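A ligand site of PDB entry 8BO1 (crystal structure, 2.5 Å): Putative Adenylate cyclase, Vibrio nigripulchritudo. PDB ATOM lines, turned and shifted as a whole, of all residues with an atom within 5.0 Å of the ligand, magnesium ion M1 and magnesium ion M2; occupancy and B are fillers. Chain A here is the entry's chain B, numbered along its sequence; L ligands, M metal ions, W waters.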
ATOM      1  N   ARG A  60     -34.094  26.429 -15.709  1.00  0.00           N
ATOM      2  CA  ARG A  60     -33.792  24.990 -15.517  1.00  0.00           C
ATOM      3  C   ARG A  60     -34.869  24.280 -14.671  1.00  0.00           C
ATOM      4  O   ARG A  60     -35.676  24.964 -14.049  1.00  0.00           O
ATOM      5  CB  ARG A  60     -32.401  24.840 -14.907  1.00  0.00           C
ATOM      6  CG  ARG A  60     -31.289  25.117 -15.910  1.00  0.00           C
ATOM      7  CD  ARG A  60     -29.891  24.867 -15.363  1.00  0.00           C
ATOM      8  NE  ARG A  60     -29.785  23.549 -14.738  1.00  0.00           N
ATOM      9  CZ  ARG A  60     -29.300  23.332 -13.519  1.00  0.00           C
ATOM     10  NH1 ARG A  60     -28.836  24.348 -12.791  1.00  0.00           N
ATOM     11  NH2 ARG A  60     -29.221  22.098 -13.034  1.00  0.00           N
ATOM     12  N   LYS A  78     -30.950  28.297  -2.324  1.00  0.00           N
ATOM     13  CA  LYS A  78     -29.496  28.122  -2.403  1.00  0.00           C
ATOM     14  C   LYS A  78     -28.805  28.918  -3.485  1.00  0.00           C
ATOM     15  O   LYS A  78     -29.114  28.784  -4.663  1.00  0.00           O
ATOM     16  CB  LYS A  78     -29.144  26.637  -2.533  1.00  0.00           C
ATOM     17  CG  LYS A  78     -29.915  25.931  -3.613  1.00  0.00           C
ATOM     18  CD  LYS A  78     -29.422  24.514  -3.861  1.00  0.00           C
ATOM     19  CE  LYS A  78     -28.166  24.481  -4.674  1.00  0.00           C
ATOM     20  NZ  LYS A  78     -27.861  23.111  -5.114  1.00  0.00           N
ATOM     21  N   LEU A  80     -24.787  30.365  -5.062  1.00  0.00           N
ATOM     22  CA  LEU A  80     -23.492  29.825  -5.475  1.00  0.00           C
ATOM     23  C   LEU A  80     -22.610  29.350  -4.312  1.00  0.00           C
ATOM     24  O   LEU A  80     -21.702  28.542  -4.536  1.00  0.00           O
ATOM     25  CB  LEU A  80     -22.736  30.862  -6.333  1.00  0.00           C
ATOM     26  CG  LEU A  80     -22.485  30.486  -7.790  1.00  0.00           C
ATOM     27  CD1 LEU A  80     -23.738  30.066  -8.464  1.00  0.00           C
ATOM     28  CD2 LEU A  80     -21.958  31.641  -8.560  1.00  0.00           C
ATOM     29  N   VAL A  82     -23.733  27.543  -1.824  1.00  0.00           N
ATOM     30  CA  VAL A  82     -24.305  26.309  -1.351  1.00  0.00           C
ATOM     31  C   VAL A  82     -24.358  25.432  -2.560  1.00  0.00           C
ATOM     32  O   VAL A  82     -25.349  25.465  -3.276  1.00  0.00           O
ATOM     33  CB  VAL A  82     -25.698  26.513  -0.692  1.00  0.00           C
ATOM     34  CG1 VAL A  82     -26.304  25.177  -0.271  1.00  0.00           C
ATOM     35  CG2 VAL A  82     -25.581  27.439   0.514  1.00  0.00           C
ATOM     36  N   LYS A  83     -23.260  24.748  -2.879  1.00  0.00           N
ATOM     37  CA  LYS A  83     -23.227  23.891  -4.069  1.00  0.00           C
ATOM     38  C   LYS A  83     -23.805  22.468  -3.843  1.00  0.00           C
ATOM     39  O   LYS A  83     -24.016  21.715  -4.796  1.00  0.00           O
ATOM     40  CB  LYS A  83     -21.824  23.852  -4.674  1.00  0.00           C
ATOM     41  CG  LYS A  83     -21.376  25.150  -5.293  1.00  0.00           C
ATOM     42  CD  LYS A  83     -19.879  25.047  -5.523  1.00  0.00           C
ATOM     43  CE  LYS A  83     -19.414  25.957  -6.613  1.00  0.00           C
ATOM     44  NZ  LYS A  83     -19.819  27.350  -6.341  1.00  0.00           N
ATOM     45  N   ALA A  84     -24.073  22.105  -2.599  1.00  0.00           N
ATOM     46  CA  ALA A  84     -24.689  20.848  -2.179  1.00  0.00           C
ATOM     47  C   ALA A  84     -26.067  20.754  -2.848  1.00  0.00           C
ATOM     48  O   ALA A  84     -26.801  21.747  -2.844  1.00  0.00           O
ATOM     49  CB  ALA A  84     -24.869  20.877  -0.662  1.00  0.00           C
ATOM     50  N   LYS A  85     -26.391  19.622  -3.482  1.00  0.00           N
ATOM     51  CA  LYS A  85     -27.674  19.503  -4.180  1.00  0.00           C
ATOM     52  C   LYS A  85     -28.851  19.304  -3.245  1.00  0.00           C
ATOM     53  O   LYS A  85     -28.705  18.819  -2.133  1.00  0.00           O
ATOM     54  CB  LYS A  85     -27.649  18.375  -5.216  1.00  0.00           C
ATOM     55  CG  LYS A  85     -26.579  18.549  -6.248  1.00  0.00           C
ATOM     56  CD  LYS A  85     -26.822  19.725  -7.162  1.00  0.00           C
ATOM     57  CE  LYS A  85     -26.030  19.593  -8.426  1.00  0.00           C
ATOM     58  NZ  LYS A  85     -25.445  20.884  -8.823  1.00  0.00           N
ATOM     59  N   SER A  86     -30.033  19.681  -3.716  1.00  0.00           N
ATOM     60  CA  SER A  86     -31.254  19.473  -2.989  1.00  0.00           C
ATOM     61  C   SER A  86     -31.662  18.009  -3.202  1.00  0.00           C
ATOM     62  O   SER A  86     -31.076  17.316  -4.033  1.00  0.00           O
ATOM     63  CB  SER A  86     -32.335  20.429  -3.484  1.00  0.00           C
ATOM     64  OG  SER A  86     -32.667  20.177  -4.834  1.00  0.00           O
ATOM     65  N   LYS A 104     -30.537  14.366  -4.589  1.00  0.00           N
ATOM     66  CA  LYS A 104     -30.859  13.833  -5.906  1.00  0.00           C
ATOM     67  C   LYS A 104     -29.653  13.041  -6.507  1.00  0.00           C
ATOM     68  O   LYS A 104     -28.528  13.122  -6.007  1.00  0.00           O
ATOM     69  CB  LYS A 104     -31.326  14.987  -6.810  1.00  0.00           C
ATOM     70  CG  LYS A 104     -30.313  16.120  -6.907  1.00  0.00           C
ATOM     71  CD  LYS A 104     -30.626  17.019  -8.046  1.00  0.00           C
ATOM     72  CE  LYS A 104     -31.173  18.316  -7.586  1.00  0.00           C
ATOM     73  NZ  LYS A 104     -30.835  19.392  -8.561  1.00  0.00           N
ATOM     74  N   ALA A 214     -34.379  24.567  -3.186  1.00  0.00           N
ATOM     75  CA  ALA A 214     -33.660  24.727  -4.442  1.00  0.00           C
ATOM     76  C   ALA A 214     -33.970  26.166  -4.997  1.00  0.00           C
ATOM     77  O   ALA A 214     -34.969  26.809  -4.617  1.00  0.00           O
ATOM     78  CB  ALA A 214     -34.165  23.706  -5.420  1.00  0.00           C
ATOM     79  N   ASP A 215     -33.100  26.664  -5.867  1.00  0.00           N
ATOM     80  CA  ASP A 215     -33.278  27.986  -6.461  1.00  0.00           C
ATOM     81  C   ASP A 215     -33.916  27.902  -7.864  1.00  0.00           C
ATOM     82  O   ASP A 215     -34.284  26.815  -8.313  1.00  0.00           O
ATOM     83  CB  ASP A 215     -31.899  28.689  -6.506  1.00  0.00           C
ATOM     84  CG  ASP A 215     -30.854  28.015  -7.373  1.00  0.00           C
ATOM     85  OD1 ASP A 215     -30.968  26.795  -7.616  1.00  0.00           O
ATOM     86  OD2 ASP A 215     -29.897  28.718  -7.789  1.00  0.00           O
ATOM     87  N   ASP A 217     -32.813  28.432 -11.535  1.00  0.00           N
ATOM     88  CA  ASP A 217     -31.571  28.634 -12.269  1.00  0.00           C
ATOM     89  C   ASP A 217     -31.872  29.099 -13.694  1.00  0.00           C
ATOM     90  O   ASP A 217     -32.476  28.343 -14.472  1.00  0.00           O
ATOM     91  CB  ASP A 217     -30.759  27.339 -12.314  1.00  0.00           C
ATOM     92  CG  ASP A 217     -30.123  26.937 -11.021  1.00  0.00           C
ATOM     93  OD1 ASP A 217     -29.042  27.474 -10.683  1.00  0.00           O
ATOM     94  OD2 ASP A 217     -30.683  26.060 -10.339  1.00  0.00           O
ATOM     95  N   LEU A 274     -22.338  35.920  -8.005  1.00  0.00           N
ATOM     96  CA  LEU A 274     -23.020  35.994  -9.286  1.00  0.00           C
ATOM     97  C   LEU A 274     -22.433  35.031 -10.321  1.00  0.00           C
ATOM     98  O   LEU A 274     -23.097  34.675 -11.272  1.00  0.00           O
ATOM     99  CB  LEU A 274     -22.926  37.427  -9.842  1.00  0.00           C
ATOM    100  CG  LEU A 274     -23.738  38.511  -9.170  1.00  0.00           C
ATOM    101  CD1 LEU A 274     -23.371  39.857  -9.708  1.00  0.00           C
ATOM    102  CD2 LEU A 274     -25.221  38.265  -9.290  1.00  0.00           C
ATOM    103  N   GLY A 275     -21.161  34.692 -10.175  1.00  0.00           N
ATOM    104  CA  GLY A 275     -20.455  33.840 -11.119  1.00  0.00           C
ATOM    105  C   GLY A 275     -20.095  34.629 -12.358  1.00  0.00           C
ATOM    106  O   GLY A 275     -19.738  35.815 -12.272  1.00  0.00           O
ATOM    107  N   MET A 276     -20.220  33.982 -13.513  1.00  0.00           N
ATOM    108  CA  MET A 276     -19.933  34.537 -14.827  1.00  0.00           C
ATOM    109  C   MET A 276     -21.231  35.134 -15.295  1.00  0.00           C
ATOM    110  O   MET A 276     -22.193  34.399 -15.497  1.00  0.00           O
ATOM    111  CB  MET A 276     -19.498  33.405 -15.741  1.00  0.00           C
ATOM    112  CG  MET A 276     -18.330  32.627 -15.179  1.00  0.00           C
ATOM    113  SD  MET A 276     -16.852  32.966 -16.156  1.00  0.00           S
ATOM    114  CE  MET A 276     -17.268  31.976 -17.668  1.00  0.00           C
ATOM    115  N   HIS A 303     -27.697  33.918  -9.346  1.00  0.00           N
ATOM    116  CA  HIS A 303     -26.456  34.026 -10.142  1.00  0.00           C
ATOM    117  C   HIS A 303     -26.687  34.080 -11.648  1.00  0.00           C
ATOM    118  O   HIS A 303     -27.835  34.227 -12.077  1.00  0.00           O
ATOM    119  CB  HIS A 303     -25.589  32.811  -9.829  1.00  0.00           C
ATOM    120  CG  HIS A 303     -26.316  31.507  -9.883  1.00  0.00           C
ATOM    121  ND1 HIS A 303     -26.275  30.699 -10.987  1.00  0.00           N
ATOM    122  CD2 HIS A 303     -27.050  30.848  -8.963  1.00  0.00           C
ATOM    123  CE1 HIS A 303     -26.961  29.611 -10.770  1.00  0.00           C
ATOM    124  NE2 HIS A 303     -27.454  29.680  -9.525  1.00  0.00           N
ATOM    125  N   GLY A 304     -25.599  33.913 -12.394  1.00  0.00           N
ATOM    126  CA  GLY A 304     -25.666  33.957 -13.865  1.00  0.00           C
ATOM    127  C   GLY A 304     -26.351  32.766 -14.484  1.00  0.00           C
ATOM    128  O   GLY A 304     -26.817  31.877 -13.757  1.00  0.00           O
ATOM    129  N   ALA A 305     -26.359  32.739 -15.811  1.00  0.00           N
ATOM    130  CA  ALA A 305     -27.113  31.683 -16.502  1.00  0.00           C
ATOM    131  C   ALA A 305     -26.236  30.492 -16.879  1.00  0.00           C
ATOM    132  O   ALA A 305     -25.002  30.612 -16.846  1.00  0.00           O
ATOM    133  CB  ALA A 305     -27.781  32.282 -17.704  1.00  0.00           C
ATOM    134  N   ASP A 306     -26.879  29.379 -17.211  1.00  0.00           N
ATOM    135  CA  ASP A 306     -26.166  28.180 -17.647  1.00  0.00           C
ATOM    136  C   ASP A 306     -25.365  28.440 -18.917  1.00  0.00           C
ATOM    137  O   ASP A 306     -24.462  27.709 -19.205  1.00  0.00           O
ATOM    138  CB  ASP A 306     -27.147  27.028 -17.801  1.00  0.00           C
ATOM    139  CG  ASP A 306     -26.476  25.688 -17.674  1.00  0.00           C
ATOM    140  OD1 ASP A 306     -25.928  25.400 -16.605  1.00  0.00           O
ATOM    141  OD2 ASP A 306     -26.529  24.909 -18.643  1.00  0.00           O
ATOM    142  N   ALA A 308     -23.212  30.650 -19.393  1.00  0.00           N
ATOM    143  CA  ALA A 308     -21.912  30.994 -18.897  1.00  0.00           C
ATOM    144  C   ALA A 308     -21.401  30.066 -17.817  1.00  0.00           C
ATOM    145  O   ALA A 308     -20.453  30.427 -17.135  1.00  0.00           O
ATOM    146  CB  ALA A 308     -21.984  32.403 -18.332  1.00  0.00           C
ATOM    147  N   ASN A 309     -22.006  28.882 -17.633  1.00  0.00           N
ATOM    148  CA  ASN A 309     -21.626  27.943 -16.600  1.00  0.00           C
ATOM    149  C   ASN A 309     -20.590  26.937 -17.121  1.00  0.00           C
ATOM    150  O   ASN A 309     -20.910  26.053 -17.898  1.00  0.00           O
ATOM    151  CB  ASN A 309     -22.862  27.248 -16.052  1.00  0.00           C
ATOM    152  CG  ASN A 309     -22.601  26.207 -14.984  1.00  0.00           C
ATOM    153  OD1 ASN A 309     -21.537  26.128 -14.378  1.00  0.00           O
ATOM    154  ND2 ASN A 309     -23.568  25.344 -14.749  1.00  0.00           N
ATOM    155  N   PRO A 310     -19.343  27.041 -16.632  1.00  0.00           N
ATOM    156  CA  PRO A 310     -18.302  26.079 -17.025  1.00  0.00           C
ATOM    157  C   PRO A 310     -18.614  24.637 -16.668  1.00  0.00           C
ATOM    158  O   PRO A 310     -18.118  23.705 -17.297  1.00  0.00           O
ATOM    159  CB  PRO A 310     -17.081  26.527 -16.203  1.00  0.00           C
ATOM    160  CG  PRO A 310     -17.328  27.884 -15.844  1.00  0.00           C
ATOM    161  CD  PRO A 310     -18.811  28.006 -15.668  1.00  0.00           C
ATOM    162  N   TYR A 311     -19.419  24.450 -15.640  1.00  0.00           N
ATOM    163  CA  TYR A 311     -19.761  23.148 -15.114  1.00  0.00           C
ATOM    164  C   TYR A 311     -21.163  22.718 -15.537  1.00  0.00           C
ATOM    165  O   TYR A 311     -21.791  21.951 -14.825  1.00  0.00           O
ATOM    166  CB  TYR A 311     -19.655  23.175 -13.575  1.00  0.00           C
ATOM    167  CG  TYR A 311     -18.365  23.828 -13.108  1.00  0.00           C
ATOM    168  CD1 TYR A 311     -17.147  23.237 -13.358  1.00  0.00           C
ATOM    169  CD2 TYR A 311     -18.376  25.086 -12.523  1.00  0.00           C
ATOM    170  CE1 TYR A 311     -15.952  23.841 -12.974  1.00  0.00           C
ATOM    171  CE2 TYR A 311     -17.195  25.703 -12.133  1.00  0.00           C
ATOM    172  CZ  TYR A 311     -15.985  25.081 -12.364  1.00  0.00           C
ATOM    173  OH  TYR A 311     -14.820  25.699 -11.979  1.00  0.00           O
HETATM  174  P1  LIG L   1     -30.764  22.166  -6.912  1.00  0.00           P
HETATM  175  O1  LIG L   1     -32.158  21.718  -7.077  1.00  0.00           O
HETATM  176  O2  LIG L   1     -30.643  23.695  -6.923  1.00  0.00           O
HETATM  177  O3  LIG L   1     -30.060  21.649  -5.680  1.00  0.00           O
HETATM  178  P2  LIG L   1     -28.994  22.322  -9.285  1.00  0.00           P
HETATM  179  O4  LIG L   1     -28.507  21.230 -10.168  1.00  0.00           O
HETATM  180  O5  LIG L   1     -29.822  23.448  -9.910  1.00  0.00           O
HETATM  181  O6  LIG L   1     -29.866  21.668  -8.126  1.00  0.00           O
HETATM  182  P3  LIG L   1     -27.242  24.511  -8.457  1.00  0.00           P
HETATM  183  O7  LIG L   1     -28.331  25.537  -8.432  1.00  0.00           O
HETATM  184  O8  LIG L   1     -26.212  24.581  -7.335  1.00  0.00           O
HETATM  185  O9  LIG L   1     -27.815  23.027  -8.479  1.00  0.00           O
HETATM  186  O10 LIG L   1     -26.543  24.461  -9.833  1.00  0.00           O
HETATM  187  C1  LIG L   1     -25.990  25.636 -10.431  1.00  0.00           C
HETATM  188  C2  LIG L   1     -24.509  25.498 -10.305  1.00  0.00           C
HETATM  189  O11 LIG L   1     -23.927  25.824 -11.590  1.00  0.00           O
HETATM  190  C3  LIG L   1     -23.881  26.476  -9.315  1.00  0.00           C
HETATM  191  C4  LIG L   1     -22.544  26.825  -9.957  1.00  0.00           C
HETATM  192  O12 LIG L   1     -21.547  25.840  -9.680  1.00  0.00           O
HETATM  193  C5  LIG L   1     -22.877  26.756 -11.446  1.00  0.00           C
HETATM  194  N1  LIG L   1     -23.258  27.993 -12.115  1.00  0.00           N
HETATM  195  C6  LIG L   1     -24.438  28.240 -12.776  1.00  0.00           C
HETATM  196  N2  LIG L   1     -24.439  29.334 -13.495  1.00  0.00           N
HETATM  197  C7  LIG L   1     -23.170  29.849 -13.297  1.00  0.00           C
HETATM  198  C8  LIG L   1     -22.495  30.938 -13.887  1.00  0.00           C
HETATM  199  N3  LIG L   1     -23.066  31.819 -14.693  1.00  0.00           N
HETATM  200  N4  LIG L   1     -21.187  31.103 -13.588  1.00  0.00           N
HETATM  201  C9  LIG L   1     -20.613  30.259 -12.717  1.00  0.00           C
HETATM  202  N5  LIG L   1     -21.158  29.222 -12.076  1.00  0.00           N
HETATM  203  C10 LIG L   1     -22.445  29.056 -12.433  1.00  0.00           C
HETATM  204 MG    MG M   1     -28.171  27.894  -8.635  1.00  0.00          MG
HETATM  205 MG    MG M   2     -30.824  24.931  -8.674  1.00  0.00          MG
HETATM  206  O   HOH W   1     -27.420  27.892  -6.636  1.00  0.00           O
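Two residues have an atom within 4 Å of magnesium ion M2: Asp 215 and Asp 217.
The backbone carbonyl oxygen (O) of Gly 304 lies close to a nitrogen (N2) of the ligand (3.5 Å).
Leu 80 touches the ligand.
CE of Lys 83 touches O12 of the ligand, at 3.7 Å.
Ala 214 touches the ligand.
Gly 275 touches the ligand (CA to N4, 3.8 Å).
Ala 308 touches the ligand.
Hydrophobic or aromatic side chains that line the ligand: Leu 80, Ala 214, Met 276, His 303 and Ala 308.
Of the 23 residues printed, 3 come within 4 Å of magnesium ion M1.
An oxygen (O1) of the ligand lies within salt-bridge range of the side-chain amino group (NZ) of Lys 104 (3.1 Å).
O3 of the ligand is in salt-bridge range of NZ of Lys 78, at 2.7 Å.
The backbone NH of Ser 86 is in hydrogen-bond range of an oxygen (O3) of the ligand (2.8 Å).
OG of Ser 86 sits at hydrogen-bond distance from O1 of the ligand (2.8 Å).
The backbone NH of Met 276 sits at hydrogen-bond distance from a nitrogen (N4) of the ligand (3.0 Å).
The backbone carbonyl oxygen (O) of Met 276 sits at hydrogen-bond distance from a nitrogen (N3) of the ligand (2.8 Å).
The guanidinium group (NH2) of Arg 60 is in salt-bridge range of an oxygen (O4) of the ligand (3.1 Å).
The backbone carbonyl oxygen (O) of Ala 305 is in hydrogen-bond range of a nitrogen (N3) of the ligand (3.1 Å).
An oxygen (O4) of the ligand is in salt-bridge range of the side-chain amino group (NZ) of Lys 85 (3.4 Å).
ND2 of Asn 309 sits at hydrogen-bond distance from O11 of the ligand, 3.2 Å away.
The backbone carbonyl oxygen (O) of Asp 217 lies within hydrogen-bond range of the backbone NH (N) of Arg 60, at 2.8 Å.
The backbone NH (N) of Lys 104 is in hydrogen-bond range of the backbone carbonyl oxygen (O) of Ser 86, at 3.0 Å.
The side-chain amino group of Lys 78 sits at hydrogen-bond distance from the backbone carbonyl oxygen of Ala 84 (2.9 Å).
The side-chain amide oxygen of Asn 309 is in hydrogen-bond range of the backbone NH of Tyr 311, at 3.0 Å.
The side-chain carboxylate (OD1) of Asp 306 sits at hydrogen-bond distance from the side-chain amide nitrogen (ND2) of Asn 309 (3.0 Å).
The backbone carbonyl oxygen of Leu 274 is in hydrogen-bond range of the backbone NH of Gly 304, 2.8 Å away.
The backbone carbonyl oxygen (O) of Leu 80 is in hydrogen-bond range of the side-chain amino group (NZ) of Lys 83 (2.9 Å).
OD2 of Asp 215 is bound to magnesium ion M1.
NE2 of His 303 binds magnesium ion M1.
Water W1 binds magnesium ion M1, at 2.1 Å.
Magnesium ion M1 is bound by OD1 of Asp 217, at 2.3 Å.
O7 of the ligand is bound to magnesium ion M1 (2.4 Å).
Magnesium ion M2 is bound by the side-chain carboxylate (OD2) of Asp 217 (2.0 Å), the side-chain carboxylate (OD1) of Asp 215 (2.1 Å), an oxygen (O2) of the ligand (2.2 Å), an oxygen (O5) of the ligand (2.2 Å) and an oxygen (O7) of the ligand (2.6 Å).
Magnesium ion M2 has five donor atoms within binding distance.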
